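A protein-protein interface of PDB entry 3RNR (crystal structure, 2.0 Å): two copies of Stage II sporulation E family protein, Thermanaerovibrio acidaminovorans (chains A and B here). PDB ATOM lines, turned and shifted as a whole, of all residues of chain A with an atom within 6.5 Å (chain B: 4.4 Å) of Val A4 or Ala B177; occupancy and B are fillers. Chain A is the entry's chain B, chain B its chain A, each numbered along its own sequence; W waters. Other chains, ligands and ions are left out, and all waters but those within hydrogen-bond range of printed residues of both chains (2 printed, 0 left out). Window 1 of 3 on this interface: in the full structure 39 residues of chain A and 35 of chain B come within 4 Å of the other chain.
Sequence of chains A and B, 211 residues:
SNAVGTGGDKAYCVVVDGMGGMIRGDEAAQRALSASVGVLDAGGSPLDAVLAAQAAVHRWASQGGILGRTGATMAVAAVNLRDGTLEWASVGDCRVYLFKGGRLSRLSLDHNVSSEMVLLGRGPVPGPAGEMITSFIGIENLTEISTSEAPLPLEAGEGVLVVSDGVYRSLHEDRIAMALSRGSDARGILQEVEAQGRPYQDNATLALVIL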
ATOM      1  N   ASN A   2     -11.849 -20.376  13.092  1.00  0.00           N
ATOM      2  CA  ASN A   2     -10.868 -19.392  13.511  1.00  0.00           C
ATOM      3  C   ASN A   2      -9.519 -19.712  12.884  1.00  0.00           C
ATOM      4  O   ASN A   2      -9.318 -20.805  12.345  1.00  0.00           O
ATOM      5  CB  ASN A   2     -10.784 -19.272  15.044  1.00  0.00           C
ATOM      6  CG  ASN A   2     -10.308 -20.552  15.711  1.00  0.00           C
ATOM      7  OD1 ASN A   2      -9.982 -21.525  15.038  1.00  0.00           O
ATOM      8  ND2 ASN A   2     -10.264 -20.552  17.044  1.00  0.00           N
ATOM      9  N   ALA A   3      -8.635 -18.726  12.874  1.00  0.00           N
ATOM     10  CA  ALA A   3      -7.281 -18.931  12.392  1.00  0.00           C
ATOM     11  C   ALA A   3      -6.383 -17.892  13.006  1.00  0.00           C
ATOM     12  O   ALA A   3      -6.835 -16.787  13.324  1.00  0.00           O
ATOM     13  CB  ALA A   3      -7.237 -18.842  10.866  1.00  0.00           C
ATOM     14  N   VAL A   4      -5.109 -18.240  13.156  1.00  0.00           N
ATOM     15  CA  VAL A   4      -4.084 -17.259  13.455  1.00  0.00           C
ATOM     16  C   VAL A   4      -2.931 -17.625  12.572  1.00  0.00           C
ATOM     17  O   VAL A   4      -2.838 -18.752  12.089  1.00  0.00           O
ATOM     18  CB  VAL A   4      -3.600 -17.282  14.933  1.00  0.00           C
ATOM     19  CG1 VAL A   4      -4.748 -16.911  15.880  1.00  0.00           C
ATOM     20  CG2 VAL A   4      -3.016 -18.644  15.285  1.00  0.00           C
ATOM     21  N   GLY A   5      -2.038 -16.675  12.367  1.00  0.00           N
ATOM     22  CA  GLY A   5      -0.920 -16.922  11.499  1.00  0.00           C
ATOM     23  C   GLY A   5       0.107 -15.829  11.566  1.00  0.00           C
ATOM     24  O   GLY A   5      -0.075 -14.797  12.216  1.00  0.00           O
ATOM     25  N   THR A   6       1.208 -16.090  10.889  1.00  0.00           N
ATOM     26  CA  THR A   6       2.300 -15.153  10.807  1.00  0.00           C
ATOM     27  C   THR A   6       2.682 -15.095   9.355  1.00  0.00           C
ATOM     28  O   THR A   6       3.112 -16.107   8.800  1.00  0.00           O
ATOM     29  CB  THR A   6       3.535 -15.663  11.583  1.00  0.00           C
ATOM     30  OG1 THR A   6       3.115 -16.405  12.732  1.00  0.00           O
ATOM     31  CG2 THR A   6       4.396 -14.494  12.026  1.00  0.00           C
ATOM     32  N   TYR A  12      -1.560 -12.387  12.897  1.00  0.00           N
ATOM     33  CA  TYR A  12      -2.974 -12.034  12.752  1.00  0.00           C
ATOM     34  C   TYR A  12      -3.870 -13.082  13.370  1.00  0.00           C
ATOM     35  O   TYR A  12      -3.445 -14.216  13.608  1.00  0.00           O
ATOM     36  CB  TYR A  12      -3.332 -11.870  11.270  1.00  0.00           C
ATOM     37  CG  TYR A  12      -3.150 -13.140  10.463  1.00  0.00           C
ATOM     38  CD1 TYR A  12      -4.121 -14.141  10.465  1.00  0.00           C
ATOM     39  CD2 TYR A  12      -2.001 -13.349   9.721  1.00  0.00           C
ATOM     40  CE1 TYR A  12      -3.949 -15.308   9.724  1.00  0.00           C
ATOM     41  CE2 TYR A  12      -1.823 -14.503   8.982  1.00  0.00           C
ATOM     42  CZ  TYR A  12      -2.791 -15.478   8.997  1.00  0.00           C
ATOM     43  OH  TYR A  12      -2.595 -16.625   8.262  1.00  0.00           O
ATOM     44  N   CYS A  13      -5.121 -12.700  13.602  1.00  0.00           N
ATOM     45  CA  CYS A  13      -6.125 -13.620  14.120  1.00  0.00           C
ATOM     46  C   CYS A  13      -7.461 -13.298  13.473  1.00  0.00           C
ATOM     47  O   CYS A  13      -7.737 -12.147  13.134  1.00  0.00           O
ATOM     48  CB  CYS A  13      -6.243 -13.502  15.640  1.00  0.00           C
ATOM     49  SG  CYS A  13      -6.579 -11.815  16.286  1.00  0.00           S
ATOM     50  N   VAL A  14      -8.281 -14.321  13.275  1.00  0.00           N
ATOM     51  CA  VAL A  14      -9.578 -14.108  12.667  1.00  0.00           C
ATOM     52  C   VAL A  14     -10.576 -15.133  13.197  1.00  0.00           C
ATOM     53  O   VAL A  14     -10.208 -16.275  13.481  1.00  0.00           O
ATOM     54  CB  VAL A  14      -9.484 -14.142  11.110  1.00  0.00           C
ATOM     55  CG1 VAL A  14      -8.715 -15.345  10.637  1.00  0.00           C
ATOM     56  CG2 VAL A  14     -10.886 -14.113  10.476  1.00  0.00           C
ATOM     57  N   VAL A  37      -7.794 -14.992   5.080  1.00  0.00           N
ATOM     58  CA  VAL A  37      -6.467 -15.538   5.383  1.00  0.00           C
ATOM     59  C   VAL A  37      -5.470 -15.332   4.239  1.00  0.00           C
ATOM     60  O   VAL A  37      -4.305 -15.024   4.472  1.00  0.00           O
ATOM     61  CB  VAL A  37      -6.533 -17.047   5.794  1.00  0.00           C
ATOM     62  CG1 VAL A  37      -5.131 -17.669   5.791  1.00  0.00           C
ATOM     63  CG2 VAL A  37      -7.173 -17.184   7.173  1.00  0.00           C
ATOM     64  N   ALA A 177      -7.370 -20.497  18.993  1.00  0.00           N
ATOM     65  CA  ALA A 177      -6.173 -20.312  18.173  1.00  0.00           C
ATOM     66  C   ALA A 177      -5.394 -19.106  18.709  1.00  0.00           C
ATOM     67  O   ALA A 177      -5.974 -18.048  18.930  1.00  0.00           O
ATOM     68  CB  ALA A 177      -6.550 -20.095  16.706  1.00  0.00           C
ATOM     69  N   MET A 178      -4.092 -19.264  18.923  1.00  0.00           N
ATOM     70  CA  MET A 178      -3.298 -18.182  19.500  1.00  0.00           C
ATOM     71  C   MET A 178      -1.970 -18.063  18.785  1.00  0.00           C
ATOM     72  O   MET A 178      -1.317 -19.068  18.511  1.00  0.00           O
ATOM     73  CB  MET A 178      -2.971 -18.455  20.978  1.00  0.00           C
ATOM     74  CG  MET A 178      -4.087 -19.005  21.823  1.00  0.00           C
ATOM     75  SD  MET A 178      -3.364 -19.470  23.599  1.00  0.00           S
ATOM     76  CE  MET A 178      -1.912 -20.625  23.045  1.00  0.00           C
ATOM     77  N   ALA A 179      -1.570 -16.826  18.519  1.00  0.00           N
ATOM     78  CA  ALA A 179      -0.239 -16.522  18.020  1.00  0.00           C
ATOM     79  C   ALA A 179       0.524 -15.825  19.143  1.00  0.00           C
ATOM     80  O   ALA A 179       0.135 -14.737  19.547  1.00  0.00           O
ATOM     81  CB  ALA A 179      -0.352 -15.608  16.808  1.00  0.00           C
ATOM     82  N   LEU A 180       1.595 -16.454  19.651  1.00  0.00           N
ATOM     83  CA  LEU A 180       2.379 -15.898  20.747  1.00  0.00           C
ATOM     84  C   LEU A 180       3.868 -15.903  20.398  1.00  0.00           C
ATOM     85  O   LEU A 180       4.278 -16.410  19.365  1.00  0.00           O
ATOM     86  CB  LEU A 180       2.207 -16.746  22.010  1.00  0.00           C
ATOM     87  CG  LEU A 180       0.844 -17.364  22.307  1.00  0.00           C
ATOM     88  CD1 LEU A 180       0.975 -18.427  23.385  1.00  0.00           C
ATOM     89  CD2 LEU A 180      -0.131 -16.275  22.739  1.00  0.00           C
ATOM     90  N   LEU A 206     -12.691 -18.362  19.728  1.00  0.00           N
ATOM     91  CA  LEU A 206     -11.718 -17.350  20.126  1.00  0.00           C
ATOM     92  C   LEU A 206     -10.452 -17.466  19.313  1.00  0.00           C
ATOM     93  O   LEU A 206     -10.017 -18.575  18.985  1.00  0.00           O
ATOM     94  CB  LEU A 206     -11.336 -17.522  21.607  1.00  0.00           C
ATOM     95  CG  LEU A 206     -12.407 -17.435  22.689  1.00  0.00           C
ATOM     96  CD1 LEU A 206     -11.774 -17.649  24.060  1.00  0.00           C
ATOM     97  CD2 LEU A 206     -13.137 -16.085  22.630  1.00  0.00           C
ATOM     98  N   ALA A 207      -9.860 -16.321  18.993  1.00  0.00           N
ATOM     99  CA  ALA A 207      -8.532 -16.287  18.404  1.00  0.00           C
ATOM    100  C   ALA A 207      -7.830 -15.062  18.948  1.00  0.00           C
ATOM    101  O   ALA A 207      -8.457 -14.020  19.188  1.00  0.00           O
ATOM    102  CB  ALA A 207      -8.594 -16.238  16.885  1.00  0.00           C
ATOM    103  N   LEU A 208      -6.525 -15.172  19.151  1.00  0.00           N
ATOM    104  CA  LEU A 208      -5.817 -14.064  19.765  1.00  0.00           C
ATOM    105  C   LEU A 208      -4.383 -13.930  19.305  1.00  0.00           C
ATOM    106  O   LEU A 208      -3.754 -14.901  18.882  1.00  0.00           O
ATOM    107  CB  LEU A 208      -5.878 -14.172  21.288  1.00  0.00           C
ATOM    108  CG  LEU A 208      -5.254 -15.415  21.881  1.00  0.00           C
ATOM    109  CD1 LEU A 208      -3.863 -15.086  22.402  1.00  0.00           C
ATOM    110  CD2 LEU A 208      -6.145 -15.932  23.009  1.00  0.00           C
ATOM    111  N   VAL A 209      -3.850 -12.727  19.411  1.00  0.00           N
ATOM    112  CA  VAL A 209      -2.447 -12.459  19.162  1.00  0.00           C
ATOM    113  C   VAL A 209      -1.839 -11.741  20.351  1.00  0.00           C
ATOM    114  O   VAL A 209      -2.446 -10.870  20.881  1.00  0.00           O
ATOM    115  CB  VAL A 209      -2.219 -11.624  17.932  1.00  0.00           C
ATOM    116  CG1 VAL A 209      -0.735 -11.371  17.728  1.00  0.00           C
ATOM    117  CG2 VAL A 209      -2.836 -12.242  16.735  1.00  0.00           C
ATOM    118  N   ASN B   2       3.313 -19.207   8.618  1.00  0.00           N
ATOM    119  CA  ASN B   2       2.557 -20.302   9.228  1.00  0.00           C
ATOM    120  C   ASN B   2       1.121 -19.907   9.522  1.00  0.00           C
ATOM    121  O   ASN B   2       0.768 -18.722   9.489  1.00  0.00           O
ATOM    122  CB  ASN B   2       3.256 -20.838  10.499  1.00  0.00           C
ATOM    123  CG  ASN B   2       3.236 -19.856  11.656  1.00  0.00           C
ATOM    124  OD1 ASN B   2       2.576 -18.822  11.607  1.00  0.00           O
ATOM    125  ND2 ASN B   2       3.961 -20.192  12.722  1.00  0.00           N
ATOM    126  N   ALA B   3       0.286 -20.911   9.751  1.00  0.00           N
ATOM    127  CA  ALA B   3      -1.080 -20.672  10.174  1.00  0.00           C
ATOM    128  C   ALA B   3      -1.591 -21.873  10.949  1.00  0.00           C
ATOM    129  O   ALA B   3      -1.146 -22.998  10.718  1.00  0.00           O
ATOM    130  CB  ALA B   3      -1.947 -20.415   8.967  1.00  0.00           C
ATOM    131  N   VAL B   4      -2.527 -21.635  11.864  1.00  0.00           N
ATOM    132  CA  VAL B   4      -3.265 -22.719  12.488  1.00  0.00           C
ATOM    133  C   VAL B   4      -4.685 -22.231  12.597  1.00  0.00           C
ATOM    134  O   VAL B   4      -4.948 -21.026  12.612  1.00  0.00           O
ATOM    135  CB  VAL B   4      -2.764 -23.110  13.912  1.00  0.00           C
ATOM    136  CG1 VAL B   4      -1.254 -23.366  13.911  1.00  0.00           C
ATOM    137  CG2 VAL B   4      -3.115 -22.047  14.902  1.00  0.00           C
ATOM    138  N   ILE B 176       5.042 -18.270  17.439  1.00  0.00           N
ATOM    139  CA  ILE B 176       4.442 -19.593  17.499  1.00  0.00           C
ATOM    140  C   ILE B 176       2.944 -19.451  17.319  1.00  0.00           C
ATOM    141  O   ILE B 176       2.336 -18.550  17.887  1.00  0.00           O
ATOM    142  CB  ILE B 176       4.704 -20.268  18.848  1.00  0.00           C
ATOM    143  CG1 ILE B 176       6.191 -20.204  19.193  1.00  0.00           C
ATOM    144  CG2 ILE B 176       4.215 -21.716  18.830  1.00  0.00           C
ATOM    145  CD1 ILE B 176       6.530 -20.806  20.538  1.00  0.00           C
ATOM    146  N   ALA B 177       2.367 -20.339  16.519  1.00  0.00           N
ATOM    147  CA  ALA B 177       0.929 -20.385  16.321  1.00  0.00           C
ATOM    148  C   ALA B 177       0.468 -21.729  16.862  1.00  0.00           C
ATOM    149  O   ALA B 177       1.096 -22.753  16.604  1.00  0.00           O
ATOM    150  CB  ALA B 177       0.600 -20.258  14.848  1.00  0.00           C
ATOM    151  N   MET B 178      -0.600 -21.726  17.646  1.00  0.00           N
ATOM    152  CA  MET B 178      -1.076 -22.972  18.233  1.00  0.00           C
ATOM    153  C   MET B 178      -2.574 -22.999  18.373  1.00  0.00           C
ATOM    154  O   MET B 178      -3.213 -21.972  18.585  1.00  0.00           O
ATOM    155  CB  MET B 178      -0.412 -23.241  19.589  1.00  0.00           C
ATOM    156  CG  MET B 178      -0.532 -22.140  20.608  1.00  0.00           C
ATOM    157  SD  MET B 178       0.757 -22.425  22.089  1.00  0.00           S
ATOM    158  CE  MET B 178       0.375 -24.291  22.464  1.00  0.00           C
ATOM    159  N   LEU B 206       7.259 -22.055  14.278  1.00  0.00           N
ATOM    160  CA  LEU B 206       6.515 -23.243  14.716  1.00  0.00           C
ATOM    161  C   LEU B 206       4.998 -23.101  14.609  1.00  0.00           C
ATOM    162  O   LEU B 206       4.447 -22.028  14.831  1.00  0.00           O
ATOM    163  CB  LEU B 206       6.858 -23.589  16.168  1.00  0.00           C
ATOM    164  CG  LEU B 206       8.339 -23.767  16.522  1.00  0.00           C
ATOM    165  CD1 LEU B 206       8.493 -23.991  18.014  1.00  0.00           C
ATOM    166  CD2 LEU B 206       8.949 -24.924  15.752  1.00  0.00           C
ATOM    167  N   ALA B 207       4.324 -24.200  14.294  1.00  0.00           N
ATOM    168  CA  ALA B 207       2.872 -24.247  14.400  1.00  0.00           C
ATOM    169  C   ALA B 207       2.508 -25.587  14.979  1.00  0.00           C
ATOM    170  O   ALA B 207       3.120 -26.601  14.641  1.00  0.00           O
ATOM    171  CB  ALA B 207       2.198 -24.055  13.047  1.00  0.00           C
ATOM    172  N   LEU B 208       1.524 -25.605  15.866  1.00  0.00           N
ATOM    173  CA  LEU B 208       1.181 -26.862  16.505  1.00  0.00           C
ATOM    174  C   LEU B 208      -0.292 -26.953  16.863  1.00  0.00           C
ATOM    175  O   LEU B 208      -0.971 -25.951  17.037  1.00  0.00           O
ATOM    176  CB  LEU B 208       2.059 -27.085  17.732  1.00  0.00           C
ATOM    177  CG  LEU B 208       1.925 -26.073  18.865  1.00  0.00           C
ATOM    178  CD1 LEU B 208       0.718 -26.423  19.712  1.00  0.00           C
ATOM    179  CD2 LEU B 208       3.175 -26.086  19.715  1.00  0.00           C
HETATM  180  O   HOH W   1      -0.099 -16.962   7.426  1.00  0.00           O
HETATM  181  O   HOH W   2       2.871 -15.656  16.610  1.00  0.00           O
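The backbone carbonyl oxygen (O) of Val B4 lies within hydrogen-bond range of the backbone NH (N) of Val A4 (2.8 Å).
The backbone NH (N) of Ile B176 sits at hydrogen-bond distance from the backbone carbonyl oxygen (O) of Leu A180 (2.8 Å).
OG1 of Thr A6 lies within hydrogen-bond range of OD1 of Asn B2.
The backbone carbonyl oxygen (O) of Met B178 sits at hydrogen-bond distance from the backbone NH (N) of Met A178, at 2.9 Å.
N of Ala A179 is in hydrogen-bond range of O of Leu A208, at 2.9 Å.
The backbone carbonyl oxygen (O) of Ala B177 sits at hydrogen-bond distance from the backbone NH (N) of Leu B208, at 3.0 Å.
ND2 of Asn B2 lies within hydrogen-bond range of O of Leu B206.
The backbone NH (N) of Val A14 lies within hydrogen-bond range of the backbone carbonyl oxygen (O) of Ala A3.
The backbone NH of Tyr A12 lies within hydrogen-bond range of the backbone carbonyl oxygen of Gly A5.
The backbone carbonyl oxygen (O) of Ala A177 lies within hydrogen-bond range of the backbone NH (N) of Leu A208, at 2.9 Å.
Among the printed residues, merely in contact across the chains: Ala A3 with Val B4, Val A4 with Ala B3, Val A4 with Ala B177, Gly A5 with Asn B2, Gly A5 with Ala B3, Tyr A12 with Ala B3, Ala A177 with Met B178, Met A178 with Ile B176, Met A178 with Ala B177 and Ala A179 with Ile B176.
Printed residues of chain B within 4 Å of Val A4: Ala B3 (3.2 Å), Val B4 (2.8 Å) and Ala B177 (3.98 Å).
Printed residues of chain A within 4 Å of Ala B177: Val A4 (3.98 Å) and Met A178 (3.4 Å).
Printed residues of chain B within 4 Å of Ala A179: Ile B176 (3.3 Å).
Of the printed residues of chain A, Ile B176 touches Met A178 (3.7 Å), Ala A179 (3.3 Å) and Leu A180 (2.8 Å).
The nearest printed residue of chain B that does not touch Val A4 is Asn B2 (4.4 Å).
The nearest printed residue of chain A that does not touch Ala B177 is Ala A179 (4.4 Å).
The nearest printed residue of chain B that does not touch Ala A177 is Val B4 (4.3 Å).
Of the 9 printed residues of chain B, 6 touch a printed residue of chain A.
Printed residues of chain B that touch a printed residue of chain A: Asn B2, Ala B3, Val B4, Ile B176, Ala B177 and Met B178.
Printed residues of chain A that touch a printed residue of chain B: Ala A3, Val A4, Gly A5, Thr A6, Tyr A12, Ala A177, Met A178, Ala A179 and Leu A180.
Ala A3 touches Val B4, and with the chains exchanged Val A4 touches Ala B3.
Val A4 touches its own counterpart, Val B4.
Val A4 touches Ala B177, but with the chains exchanged Ala A177 does not touch Val B4 (4.3 Å).
Met A178 touches its own counterpart, Met B178.
Positions printed for both chains: 2, 3, 4, 177, 178, 206, 207 and 208.
Of the 14 pairs that touch across the chains among the printed residues, 6 have their exchanged pair printed and touching as well.
Water W1 bridges the side-chain hydroxyl of Tyr A12 (2.7 Å) and the backbone carbonyl oxygen of Asn B2 (2.8 Å).
Water W2 lies within hydrogen-bond range of the backbone carbonyl oxygen of Leu A180 (3.2 Å) and the backbone carbonyl oxygen of Ile B176 (3.2 Å).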
